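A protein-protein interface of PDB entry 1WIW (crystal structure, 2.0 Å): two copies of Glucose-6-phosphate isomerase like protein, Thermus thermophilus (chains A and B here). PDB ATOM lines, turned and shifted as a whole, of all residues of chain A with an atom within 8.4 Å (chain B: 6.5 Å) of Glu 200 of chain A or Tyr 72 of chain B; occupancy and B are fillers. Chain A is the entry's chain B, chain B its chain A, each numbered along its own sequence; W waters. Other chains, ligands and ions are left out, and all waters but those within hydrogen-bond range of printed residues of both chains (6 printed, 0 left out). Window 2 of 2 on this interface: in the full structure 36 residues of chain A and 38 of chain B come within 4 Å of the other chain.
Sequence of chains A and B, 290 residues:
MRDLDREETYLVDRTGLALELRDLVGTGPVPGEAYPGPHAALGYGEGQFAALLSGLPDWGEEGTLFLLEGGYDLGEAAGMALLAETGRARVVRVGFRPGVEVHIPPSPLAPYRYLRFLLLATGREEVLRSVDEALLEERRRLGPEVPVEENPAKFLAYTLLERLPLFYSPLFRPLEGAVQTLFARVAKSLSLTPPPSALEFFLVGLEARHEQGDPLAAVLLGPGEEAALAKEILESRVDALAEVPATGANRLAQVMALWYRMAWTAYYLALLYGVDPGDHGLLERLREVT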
ATOM      1  N   TYR A 168      -3.209  21.619  10.401  1.00  0.00           N
ATOM      2  CA  TYR A 168      -2.900  20.751  11.538  1.00  0.00           C
ATOM      3  C   TYR A 168      -4.218  20.297  12.180  1.00  0.00           C
ATOM      4  O   TYR A 168      -5.005  21.124  12.642  1.00  0.00           O
ATOM      5  CB  TYR A 168      -2.050  21.507  12.564  1.00  0.00           C
ATOM      6  CG  TYR A 168      -1.665  20.685  13.778  1.00  0.00           C
ATOM      7  CD1 TYR A 168      -1.729  21.231  15.060  1.00  0.00           C
ATOM      8  CD2 TYR A 168      -1.257  19.356  13.648  1.00  0.00           C
ATOM      9  CE1 TYR A 168      -1.401  20.471  16.187  1.00  0.00           C
ATOM     10  CE2 TYR A 168      -0.928  18.589  14.767  1.00  0.00           C
ATOM     11  CZ  TYR A 168      -1.005  19.155  16.032  1.00  0.00           C
ATOM     12  OH  TYR A 168      -0.713  18.392  17.142  1.00  0.00           O
ATOM     13  N   PRO A 194       2.159  19.134   8.728  1.00  0.00           N
ATOM     14  CA  PRO A 194       3.357  18.902   9.537  1.00  0.00           C
ATOM     15  C   PRO A 194       3.621  17.400   9.586  1.00  0.00           C
ATOM     16  O   PRO A 194       2.767  16.602   9.206  1.00  0.00           O
ATOM     17  CB  PRO A 194       2.970  19.470  10.895  1.00  0.00           C
ATOM     18  CG  PRO A 194       1.494  19.195  10.956  1.00  0.00           C
ATOM     19  CD  PRO A 194       1.027  19.567   9.566  1.00  0.00           C
ATOM     20  N   PRO A 195       4.818  16.998  10.022  1.00  0.00           N
ATOM     21  CA  PRO A 195       5.133  15.570  10.103  1.00  0.00           C
ATOM     22  C   PRO A 195       4.470  14.953  11.340  1.00  0.00           C
ATOM     23  O   PRO A 195       3.761  15.638  12.078  1.00  0.00           O
ATOM     24  CB  PRO A 195       6.662  15.570  10.188  1.00  0.00           C
ATOM     25  CG  PRO A 195       6.944  16.833  10.940  1.00  0.00           C
ATOM     26  CD  PRO A 195       6.020  17.818  10.263  1.00  0.00           C
ATOM     27  N   PRO A 196       4.671  13.645  11.570  1.00  0.00           N
ATOM     28  CA  PRO A 196       4.076  12.992  12.738  1.00  0.00           C
ATOM     29  C   PRO A 196       4.317  13.758  14.039  1.00  0.00           C
ATOM     30  O   PRO A 196       3.386  13.962  14.815  1.00  0.00           O
ATOM     31  CB  PRO A 196       4.737  11.628  12.725  1.00  0.00           C
ATOM     32  CG  PRO A 196       4.781  11.331  11.254  1.00  0.00           C
ATOM     33  CD  PRO A 196       5.260  12.643  10.658  1.00  0.00           C
ATOM     34  N   SER A 197       5.564  14.165  14.282  1.00  0.00           N
ATOM     35  CA  SER A 197       5.901  14.939  15.477  1.00  0.00           C
ATOM     36  C   SER A 197       5.639  16.390  15.102  1.00  0.00           C
ATOM     37  O   SER A 197       6.571  17.158  14.855  1.00  0.00           O
ATOM     38  CB  SER A 197       7.381  14.767  15.852  1.00  0.00           C
ATOM     39  OG  SER A 197       7.685  13.426  16.191  1.00  0.00           O
ATOM     40  N   ALA A 198       4.362  16.755  15.056  1.00  0.00           N
ATOM     41  CA  ALA A 198       3.959  18.096  14.657  1.00  0.00           C
ATOM     42  C   ALA A 198       4.436  19.264  15.518  1.00  0.00           C
ATOM     43  O   ALA A 198       4.970  20.241  14.994  1.00  0.00           O
ATOM     44  CB  ALA A 198       2.441  18.148  14.518  1.00  0.00           C
ATOM     45  N   LEU A 199       4.245  19.179  16.829  1.00  0.00           N
ATOM     46  CA  LEU A 199       4.638  20.281  17.701  1.00  0.00           C
ATOM     47  C   LEU A 199       6.144  20.570  17.672  1.00  0.00           C
ATOM     48  O   LEU A 199       6.555  21.726  17.690  1.00  0.00           O
ATOM     49  CB  LEU A 199       4.161  20.014  19.134  1.00  0.00           C
ATOM     50  CG  LEU A 199       2.647  19.780  19.269  1.00  0.00           C
ATOM     51  CD1 LEU A 199       2.278  19.626  20.736  1.00  0.00           C
ATOM     52  CD2 LEU A 199       1.879  20.946  18.655  1.00  0.00           C
ATOM     53  N   GLU A 200       6.961  19.525  17.625  1.00  0.00           N
ATOM     54  CA  GLU A 200       8.411  19.712  17.569  1.00  0.00           C
ATOM     55  C   GLU A 200       8.736  20.474  16.283  1.00  0.00           C
ATOM     56  O   GLU A 200       9.584  21.365  16.266  1.00  0.00           O
ATOM     57  CB  GLU A 200       9.123  18.354  17.569  1.00  0.00           C
ATOM     58  CG  GLU A 200       8.879  17.526  18.828  1.00  0.00           C
ATOM     59  CD  GLU A 200       9.646  18.037  20.035  1.00  0.00           C
ATOM     60  OE1 GLU A 200      10.127  19.191  19.997  1.00  0.00           O
ATOM     61  OE2 GLU A 200       9.759  17.286  21.030  1.00  0.00           O
ATOM     62  N   PHE A 201       8.039  20.104  15.212  1.00  0.00           N
ATOM     63  CA  PHE A 201       8.205  20.717  13.904  1.00  0.00           C
ATOM     64  C   PHE A 201       7.915  22.222  13.974  1.00  0.00           C
ATOM     65  O   PHE A 201       8.682  23.045  13.455  1.00  0.00           O
ATOM     66  CB  PHE A 201       7.251  20.034  12.919  1.00  0.00           C
ATOM     67  CG  PHE A 201       7.224  20.653  11.552  1.00  0.00           C
ATOM     68  CD1 PHE A 201       8.265  20.447  10.655  1.00  0.00           C
ATOM     69  CD2 PHE A 201       6.138  21.423  11.151  1.00  0.00           C
ATOM     70  CE1 PHE A 201       8.226  20.996   9.373  1.00  0.00           C
ATOM     71  CE2 PHE A 201       6.087  21.979   9.872  1.00  0.00           C
ATOM     72  CZ  PHE A 201       7.136  21.763   8.983  1.00  0.00           C
ATOM     73  N   PHE A 202       6.809  22.577  14.623  1.00  0.00           N
ATOM     74  CA  PHE A 202       6.420  23.978  14.752  1.00  0.00           C
ATOM     75  C   PHE A 202       7.484  24.792  15.492  1.00  0.00           C
ATOM     76  O   PHE A 202       7.727  25.947  15.165  1.00  0.00           O
ATOM     77  CB  PHE A 202       5.090  24.085  15.501  1.00  0.00           C
ATOM     78  CG  PHE A 202       3.937  23.400  14.811  1.00  0.00           C
ATOM     79  CD1 PHE A 202       2.828  22.989  15.543  1.00  0.00           C
ATOM     80  CD2 PHE A 202       3.949  23.188  13.433  1.00  0.00           C
ATOM     81  CE1 PHE A 202       1.739  22.374  14.913  1.00  0.00           C
ATOM     82  CE2 PHE A 202       2.867  22.574  12.793  1.00  0.00           C
ATOM     83  CZ  PHE A 202       1.758  22.167  13.537  1.00  0.00           C
ATOM     84  N   LEU A 203       8.107  24.170  16.487  1.00  0.00           N
ATOM     85  CA  LEU A 203       9.130  24.812  17.309  1.00  0.00           C
ATOM     86  C   LEU A 203      10.457  25.114  16.628  1.00  0.00           C
ATOM     87  O   LEU A 203      11.012  26.193  16.816  1.00  0.00           O
ATOM     88  CB  LEU A 203       9.417  23.957  18.546  1.00  0.00           C
ATOM     89  CG  LEU A 203       8.394  23.937  19.678  1.00  0.00           C
ATOM     90  CD1 LEU A 203       8.720  22.812  20.643  1.00  0.00           C
ATOM     91  CD2 LEU A 203       8.403  25.284  20.399  1.00  0.00           C
ATOM     92  N   VAL A 204      10.966  24.176  15.838  1.00  0.00           N
ATOM     93  CA  VAL A 204      12.266  24.370  15.197  1.00  0.00           C
ATOM     94  C   VAL A 204      12.294  24.639  13.697  1.00  0.00           C
ATOM     95  O   VAL A 204      13.194  25.324  13.206  1.00  0.00           O
ATOM     96  CB  VAL A 204      13.192  23.163  15.476  1.00  0.00           C
ATOM     97  CG1 VAL A 204      13.503  23.078  16.963  1.00  0.00           C
ATOM     98  CG2 VAL A 204      12.527  21.881  15.009  1.00  0.00           C
ATOM     99  N   GLY A 205      11.316  24.118  12.966  1.00  0.00           N
ATOM    100  CA  GLY A 205      11.315  24.304  11.527  1.00  0.00           C
ATOM    101  C   GLY A 205      10.693  25.557  10.937  1.00  0.00           C
ATOM    102  O   GLY A 205      10.797  25.775   9.730  1.00  0.00           O
ATOM    103  N   LEU A 206      10.065  26.393  11.760  1.00  0.00           N
ATOM    104  CA  LEU A 206       9.415  27.594  11.238  1.00  0.00           C
ATOM    105  C   LEU A 206      10.064  28.921  11.625  1.00  0.00           C
ATOM    106  O   LEU A 206       9.521  29.668  12.439  1.00  0.00           O
ATOM    107  CB  LEU A 206       7.946  27.611  11.667  1.00  0.00           C
ATOM    108  CG  LEU A 206       7.137  26.354  11.345  1.00  0.00           C
ATOM    109  CD1 LEU A 206       5.705  26.533  11.823  1.00  0.00           C
ATOM    110  CD2 LEU A 206       7.172  26.091   9.850  1.00  0.00           C
ATOM    111  N   ILE A 233       2.618  28.061  20.226  1.00  0.00           N
ATOM    112  CA  ILE A 233       3.876  27.993  19.493  1.00  0.00           C
ATOM    113  C   ILE A 233       3.847  28.772  18.172  1.00  0.00           C
ATOM    114  O   ILE A 233       4.719  29.604  17.909  1.00  0.00           O
ATOM    115  CB  ILE A 233       4.259  26.519  19.209  1.00  0.00           C
ATOM    116  CG1 ILE A 233       4.567  25.811  20.533  1.00  0.00           C
ATOM    117  CG2 ILE A 233       5.454  26.453  18.258  1.00  0.00           C
ATOM    118  CD1 ILE A 233       4.760  24.313  20.413  1.00  0.00           C
ATOM    119  N   ARG A 237       5.259  32.634  15.389  1.00  0.00           N
ATOM    120  CA  ARG A 237       6.047  32.159  14.259  1.00  0.00           C
ATOM    121  C   ARG A 237       5.451  32.232  12.854  1.00  0.00           C
ATOM    122  O   ARG A 237       6.190  32.136  11.877  1.00  0.00           O
ATOM    123  CB  ARG A 237       6.515  30.729  14.552  1.00  0.00           C
ATOM    124  CG  ARG A 237       7.378  30.619  15.815  1.00  0.00           C
ATOM    125  CD  ARG A 237       7.803  29.181  16.092  1.00  0.00           C
ATOM    126  NE  ARG A 237       8.747  29.078  17.205  1.00  0.00           N
ATOM    127  CZ  ARG A 237       8.434  29.251  18.487  1.00  0.00           C
ATOM    128  NH1 ARG A 237       7.191  29.539  18.849  1.00  0.00           N
ATOM    129  NH2 ARG A 237       9.372  29.134  19.415  1.00  0.00           N
ATOM    130  N   TYR B  44       6.505   6.365  19.130  1.00  0.00           N
ATOM    131  CA  TYR B  44       6.218   7.782  19.321  1.00  0.00           C
ATOM    132  C   TYR B  44       7.533   8.527  19.155  1.00  0.00           C
ATOM    133  O   TYR B  44       8.596   7.998  19.490  1.00  0.00           O
ATOM    134  CB  TYR B  44       5.675   8.034  20.732  1.00  0.00           C
ATOM    135  CG  TYR B  44       4.368   7.337  21.018  1.00  0.00           C
ATOM    136  CD1 TYR B  44       3.152   7.951  20.730  1.00  0.00           C
ATOM    137  CD2 TYR B  44       4.347   6.048  21.553  1.00  0.00           C
ATOM    138  CE1 TYR B  44       1.939   7.299  20.970  1.00  0.00           C
ATOM    139  CE2 TYR B  44       3.140   5.386  21.796  1.00  0.00           C
ATOM    140  CZ  TYR B  44       1.944   6.018  21.502  1.00  0.00           C
ATOM    141  OH  TYR B  44       0.753   5.368  21.729  1.00  0.00           O
ATOM    142  N   GLY B  45       7.457   9.751  18.641  1.00  0.00           N
ATOM    143  CA  GLY B  45       8.662  10.536  18.444  1.00  0.00           C
ATOM    144  C   GLY B  45       9.693   9.807  17.601  1.00  0.00           C
ATOM    145  O   GLY B  45       9.387   9.324  16.508  1.00  0.00           O
ATOM    146  N   GLU B  46      10.911   9.710  18.128  1.00  0.00           N
ATOM    147  CA  GLU B  46      12.029   9.068  17.442  1.00  0.00           C
ATOM    148  C   GLU B  46      11.836   7.581  17.177  1.00  0.00           C
ATOM    149  O   GLU B  46      12.657   6.959  16.508  1.00  0.00           O
ATOM    150  CB  GLU B  46      13.318   9.279  18.249  1.00  0.00           C
ATOM    151  CG  GLU B  46      13.657  10.746  18.454  1.00  0.00           C
ATOM    152  CD  GLU B  46      14.767  10.974  19.458  1.00  0.00           C
ATOM    153  OE1 GLU B  46      15.105  10.031  20.205  1.00  0.00           O
ATOM    154  OE2 GLU B  46      15.290  12.109  19.509  1.00  0.00           O
ATOM    155  N   GLY B  70      10.000   7.230  21.970  1.00  0.00           N
ATOM    156  CA  GLY B  70      11.180   8.008  21.636  1.00  0.00           C
ATOM    157  C   GLY B  70      11.137   9.488  21.944  1.00  0.00           C
ATOM    158  O   GLY B  70      10.074  10.058  22.187  1.00  0.00           O
ATOM    159  N   GLY B  71      12.315  10.110  21.929  1.00  0.00           N
ATOM    160  CA  GLY B  71      12.420  11.530  22.202  1.00  0.00           C
ATOM    161  C   GLY B  71      11.758  12.368  21.128  1.00  0.00           C
ATOM    162  O   GLY B  71      11.316  11.844  20.102  1.00  0.00           O
ATOM    163  N   TYR B  72      11.698  13.674  21.362  1.00  0.00           N
ATOM    164  CA  TYR B  72      11.078  14.596  20.423  1.00  0.00           C
ATOM    165  C   TYR B  72       9.666  14.138  20.094  1.00  0.00           C
ATOM    166  O   TYR B  72       9.286  14.018  18.929  1.00  0.00           O
ATOM    167  CB  TYR B  72      11.921  14.702  19.151  1.00  0.00           C
ATOM    168  CG  TYR B  72      12.916  15.838  19.204  1.00  0.00           C
ATOM    169  CD1 TYR B  72      13.861  15.916  20.229  1.00  0.00           C
ATOM    170  CD2 TYR B  72      12.887  16.860  18.255  1.00  0.00           C
ATOM    171  CE1 TYR B  72      14.750  16.988  20.310  1.00  0.00           C
ATOM    172  CE2 TYR B  72      13.770  17.933  18.325  1.00  0.00           C
ATOM    173  CZ  TYR B  72      14.698  17.992  19.355  1.00  0.00           C
ATOM    174  OH  TYR B  72      15.568  19.055  19.432  1.00  0.00           O
ATOM    175  N   ASP B  73       8.892  13.893  21.146  1.00  0.00           N
ATOM    176  CA  ASP B  73       7.517  13.427  21.013  1.00  0.00           C
ATOM    177  C   ASP B  73       6.576  14.438  21.660  1.00  0.00           C
ATOM    178  O   ASP B  73       5.491  14.081  22.122  1.00  0.00           O
ATOM    179  CB  ASP B  73       7.370  12.086  21.727  1.00  0.00           C
ATOM    180  CG  ASP B  73       7.435  12.229  23.237  1.00  0.00           C
ATOM    181  OD1 ASP B  73       8.290  12.996  23.725  1.00  0.00           O
ATOM    182  OD2 ASP B  73       6.637  11.575  23.937  1.00  0.00           O
ATOM    183  N   LEU B  74       7.002  15.695  21.695  1.00  0.00           N
ATOM    184  CA  LEU B  74       6.212  16.757  22.307  1.00  0.00           C
ATOM    185  C   LEU B  74       4.714  16.634  22.055  1.00  0.00           C
ATOM    186  O   LEU B  74       4.255  16.677  20.910  1.00  0.00           O
ATOM    187  CB  LEU B  74       6.699  18.127  21.826  1.00  0.00           C
ATOM    188  CG  LEU B  74       6.008  19.325  22.480  1.00  0.00           C
ATOM    189  CD1 LEU B  74       6.166  19.249  23.985  1.00  0.00           C
ATOM    190  CD2 LEU B  74       6.599  20.615  21.946  1.00  0.00           C
ATOM    191  N   GLY B  75       3.965  16.469  23.145  1.00  0.00           N
ATOM    192  CA  GLY B  75       2.518  16.358  23.079  1.00  0.00           C
ATOM    193  C   GLY B  75       1.909  15.158  22.371  1.00  0.00           C
ATOM    194  O   GLY B  75       0.739  15.210  21.999  1.00  0.00           O
ATOM    195  N   GLU B  76       2.667  14.081  22.189  1.00  0.00           N
ATOM    196  CA  GLU B  76       2.131  12.903  21.507  1.00  0.00           C
ATOM    197  C   GLU B  76       1.494  11.881  22.450  1.00  0.00           C
ATOM    198  O   GLU B  76       1.046  10.821  22.010  1.00  0.00           O
ATOM    199  CB  GLU B  76       3.222  12.214  20.684  1.00  0.00           C
ATOM    200  CG  GLU B  76       3.944  13.133  19.717  1.00  0.00           C
ATOM    201  CD  GLU B  76       4.745  12.371  18.682  1.00  0.00           C
ATOM    202  OE1 GLU B  76       5.379  11.356  19.042  1.00  0.00           O
ATOM    203  OE2 GLU B  76       4.748  12.794  17.507  1.00  0.00           O
ATOM    204  N   PHE B  96      13.631   7.267  25.896  1.00  0.00           N
ATOM    205  CA  PHE B  96      14.535   8.177  26.585  1.00  0.00           C
ATOM    206  C   PHE B  96      14.209   8.400  28.062  1.00  0.00           C
ATOM    207  O   PHE B  96      15.083   8.772  28.836  1.00  0.00           O
ATOM    208  CB  PHE B  96      14.553   9.528  25.857  1.00  0.00           C
ATOM    209  CG  PHE B  96      13.311  10.350  26.065  1.00  0.00           C
ATOM    210  CD1 PHE B  96      13.220  11.238  27.131  1.00  0.00           C
ATOM    211  CD2 PHE B  96      12.234  10.238  25.193  1.00  0.00           C
ATOM    212  CE1 PHE B  96      12.072  12.003  27.325  1.00  0.00           C
ATOM    213  CE2 PHE B  96      11.084  10.993  25.376  1.00  0.00           C
ATOM    214  CZ  PHE B  96      11.001  11.879  26.445  1.00  0.00           C
ATOM    215  N   PRO B 106      17.780  10.773  23.329  1.00  0.00           N
ATOM    216  CA  PRO B 106      17.217  11.458  22.163  1.00  0.00           C
ATOM    217  C   PRO B 106      18.294  11.884  21.164  1.00  0.00           C
ATOM    218  O   PRO B 106      19.377  12.323  21.553  1.00  0.00           O
ATOM    219  CB  PRO B 106      16.469  12.639  22.787  1.00  0.00           C
ATOM    220  CG  PRO B 106      17.258  12.924  24.024  1.00  0.00           C
ATOM    221  CD  PRO B 106      17.557  11.545  24.563  1.00  0.00           C
ATOM    222  N   SER B 107      17.992  11.727  19.878  1.00  0.00           N
ATOM    223  CA  SER B 107      18.917  12.083  18.797  1.00  0.00           C
ATOM    224  C   SER B 107      18.181  12.095  17.463  1.00  0.00           C
ATOM    225  O   SER B 107      17.275  11.295  17.243  1.00  0.00           O
ATOM    226  CB  SER B 107      20.068  11.070  18.715  1.00  0.00           C
ATOM    227  OG  SER B 107      20.810  11.224  17.512  1.00  0.00           O
ATOM    228  N   THR B 181      10.997  15.785   9.022  1.00  0.00           N
ATOM    229  CA  THR B 181      11.373  15.909  10.422  1.00  0.00           C
ATOM    230  C   THR B 181      12.870  16.193  10.539  1.00  0.00           C
ATOM    231  O   THR B 181      13.289  17.033  11.334  1.00  0.00           O
ATOM    232  CB  THR B 181      11.013  14.622  11.183  1.00  0.00           C
ATOM    233  OG1 THR B 181       9.590  14.566  11.337  1.00  0.00           O
ATOM    234  CG2 THR B 181      11.690  14.576  12.559  1.00  0.00           C
ATOM    235  N   ALA B 184      13.629  19.771   9.659  1.00  0.00           N
ATOM    236  CA  ALA B 184      13.171  20.727  10.659  1.00  0.00           C
ATOM    237  C   ALA B 184      14.134  20.679  11.852  1.00  0.00           C
ATOM    238  O   ALA B 184      14.708  21.693  12.253  1.00  0.00           O
ATOM    239  CB  ALA B 184      11.753  20.374  11.120  1.00  0.00           C
ATOM    240  N   ARG B 185      14.316  19.484  12.396  1.00  0.00           N
ATOM    241  CA  ARG B 185      15.171  19.280  13.565  1.00  0.00           C
ATOM    242  C   ARG B 185      16.645  19.598  13.367  1.00  0.00           C
ATOM    243  O   ARG B 185      17.273  20.194  14.241  1.00  0.00           O
ATOM    244  CB  ARG B 185      15.038  17.843  14.067  1.00  0.00           C
ATOM    245  CG  ARG B 185      15.806  17.563  15.351  1.00  0.00           C
ATOM    246  CD  ARG B 185      15.487  16.175  15.891  1.00  0.00           C
ATOM    247  NE  ARG B 185      16.154  15.904  17.163  1.00  0.00           N
ATOM    248  CZ  ARG B 185      15.970  14.795  17.877  1.00  0.00           C
ATOM    249  NH1 ARG B 185      16.615  14.621  19.023  1.00  0.00           N
ATOM    250  NH2 ARG B 185      15.140  13.856  17.439  1.00  0.00           N
ATOM    251  N   GLY B 278      22.689  20.869  15.648  1.00  0.00           N
ATOM    252  CA  GLY B 278      22.315  20.170  16.868  1.00  0.00           C
ATOM    253  C   GLY B 278      21.017  20.617  17.506  1.00  0.00           C
ATOM    254  O   GLY B 278      20.419  21.608  17.088  1.00  0.00           O
ATOM    255  N   ASP B 279      20.578  19.884  18.525  1.00  0.00           N
ATOM    256  CA  ASP B 279      19.342  20.216  19.225  1.00  0.00           C
ATOM    257  C   ASP B 279      19.566  21.336  20.235  1.00  0.00           C
ATOM    258  O   ASP B 279      20.675  21.523  20.726  1.00  0.00           O
ATOM    259  CB  ASP B 279      18.792  18.993  19.965  1.00  0.00           C
ATOM    260  CG  ASP B 279      18.438  17.849  19.035  1.00  0.00           C
ATOM    261  OD1 ASP B 279      17.915  18.109  17.931  1.00  0.00           O
ATOM    262  OD2 ASP B 279      18.667  16.683  19.419  1.00  0.00           O
ATOM    263  N   HIS B 280      18.508  22.080  20.540  1.00  0.00           N
ATOM    264  CA  HIS B 280      18.599  23.162  21.517  1.00  0.00           C
ATOM    265  C   HIS B 280      18.574  22.513  22.902  1.00  0.00           C
ATOM    266  O   HIS B 280      18.108  21.387  23.050  1.00  0.00           O
ATOM    267  CB  HIS B 280      17.384  24.095  21.418  1.00  0.00           C
ATOM    268  CG  HIS B 280      17.080  24.576  20.032  1.00  0.00           C
ATOM    269  ND1 HIS B 280      15.906  25.230  19.720  1.00  0.00           N
ATOM    270  CD2 HIS B 280      17.796  24.523  18.883  1.00  0.00           C
ATOM    271  CE1 HIS B 280      15.913  25.559  18.440  1.00  0.00           C
ATOM    272  NE2 HIS B 280      17.048  25.142  17.910  1.00  0.00           N
ATOM    273  N   LEU B 282      16.849  21.973  26.146  1.00  0.00           N
ATOM    274  CA  LEU B 282      15.465  22.204  26.554  1.00  0.00           C
ATOM    275  C   LEU B 282      15.222  22.617  28.001  1.00  0.00           C
ATOM    276  O   LEU B 282      14.080  22.880  28.381  1.00  0.00           O
ATOM    277  CB  LEU B 282      14.613  20.972  26.236  1.00  0.00           C
ATOM    278  CG  LEU B 282      14.486  20.624  24.749  1.00  0.00           C
ATOM    279  CD1 LEU B 282      13.656  19.357  24.582  1.00  0.00           C
ATOM    280  CD2 LEU B 282      13.845  21.787  24.007  1.00  0.00           C
HETATM  281  O   HOH W   1       7.986  13.212  12.967  1.00  0.00           O
HETATM  282  O   HOH W   2       5.666  16.985  18.394  1.00  0.00           O
HETATM  283  O   HOH W   3       7.815  11.083  14.870  1.00  0.00           O
HETATM  284  O   HOH W   4       9.135  16.716  13.892  1.00  0.00           O
HETATM  285  O   HOH W   5      10.612  13.031  17.021  1.00  0.00           O
HETATM  286  O   HOH W   6       5.681  10.884  16.060  1.00  0.00           O
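OE2 of Glu 200 of chain A is in hydrogen-bond range of N of Leu 74 of chain B (3.3 Å).
O of Tyr 72 of chain B lies within hydrogen-bond range of OG of Ser 197 of chain A (3.2 Å).
The side-chain carboxylate (OE2) of Glu 76 of chain B sits close to the backbone carbonyl oxygen (O) of Pro 196 of chain A (3.2 Å).
The side-chain carboxylate (OE2) of Glu 76 of chain B sits close to the side-chain hydroxyl (OG) of Ser 197 of chain A.
Water W5 lies within hydrogen-bond range of the backbone carbonyl oxygen (O) of Tyr 72 of chain B, the side-chain hydroxyl (OG) of Ser 197 of chain A and the backbone carbonyl oxygen (O) of Gly 71 of chain B.
Water W6 lies within hydrogen-bond range of the side-chain carboxylate (OE2) of Glu 76 of chain B (2.6 Å), the side-chain hydroxyl (OG) of Ser 197 of chain A (3.2 Å) and the backbone NH (N) of Gly 45 of chain B (3.3 Å).
Water W1 bridges OG1 of Thr 181 of chain B and N of Ser 197 of chain A.
Water W3 bridges the side-chain hydroxyl of Ser 197 of chain A (2.7 Å) and the backbone carbonyl oxygen of Gly 45 of chain B (2.9 Å).
Water W4 lies within hydrogen-bond range of O of Ser 197 of chain A (2.8 Å) and OG1 of Thr 181 of chain B (3.4 Å).
Water W2 lies within hydrogen-bond range of O of Leu 74 of chain B (2.9 Å), N of Glu 200 of chain A (3.0 Å) and N of Leu 199 of chain A (3.0 Å).
The side-chain hydroxyl of Tyr 72 of chain B sits at hydrogen-bond distance from the side-chain carboxylate of Asp 279 of chain B (2.9 Å).
The guanidinium group of Arg 185 of chain B lies within hydrogen-bond range of the backbone carbonyl oxygen of Ser 107 of chain B.
The side-chain carboxylate of Asp 279 of chain B is in salt-bridge range of the guanidinium group of Arg 185 of chain B.
The side-chain carboxylate of Glu 46 of chain B lies within salt-bridge range of the guanidinium group of Arg 185 of chain B (2.7 Å).
OE1 of Glu 76 of chain B is in hydrogen-bond range of N of Gly 45 of chain B, at 2.7 Å.
Printed residues of chain B that touch a printed residue of chain A: Gly 45, Tyr 72, Asp 73, Leu 74, Glu 76, Thr 181, Ala 184, Arg 185 and His 280.
Hydrophobic or aromatic side chains of chain B within 4 Å of the printed part of chain A: Tyr 72, Leu 74, Ala 184 and His 280.
Among the printed residues, 15 pairs touch across the chains.
Among the printed residues, no Asp or Glu carboxylate lies within 4 Å of a Lys or Arg side-chain nitrogen of the other chain.
No position is printed for both chains.
Of chain B, only Tyr 72 (3.1 Å), Asp 73 (3.5 Å) and Leu 74 (3.3 Å) come within 4 Å of Glu 200 of chain A.
Gly 71 of chain B touches none of the printed residues of chain A.
Of the printed residues of chain B, Ser 197 of chain A touches Gly 45 (3.8 Å), Tyr 72 (3.2 Å) and Glu 76 (3.2 Å).
Of the printed residues of chain A, Arg 185 of chain B touches Val 204.
Printed residues of chain A within 4 Å of Leu 74 of chain B: Leu 199 (3.6 Å), Glu 200 (3.3 Å) and Leu 203 (3.3 Å).
Of the printed residues of chain A, Glu 76 of chain B touches Pro 196 and Ser 197.
Of the printed residues of chain B, Val 204 of chain A touches Ala 184 (3.5 Å), Arg 185 (3.97 Å) and His 280 (3.8 Å).
Asp 279 of chain B touches none of the printed residues of chain A.
Gly 278 of chain B touches none of the printed residues of chain A.
The nearest printed residue of chain B that does not touch Leu 199 of chain A is Gly 75 of chain B (4.03 Å).
Among the printed residues, merely in contact across the chains: Glu 200 of chain A with Tyr 72 of chain B (3.1 Å), Pro 195 of chain A with Thr 181 of chain B (3.3 Å), Leu 203 of chain A with Leu 74 of chain B (3.3 Å), Glu 200 of chain A with Asp 73 of chain B (3.5 Å), Val 204 of chain A with Ala 184 of chain B (3.5 Å), Phe 201 of chain A with Ala 184 of chain B (3.5 Å), Leu 199 of chain A with Leu 74 of chain B (3.6 Å), Val 204 of chain A with His 280 of chain B (3.8 Å), Ser 197 of chain A with Gly 45 of chain B (3.8 Å), Val 204 of chain A with Arg 185 of chain B (3.97 Å) and Gly 205 of chain A with Ala 184 of chain B (3.98 Å).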
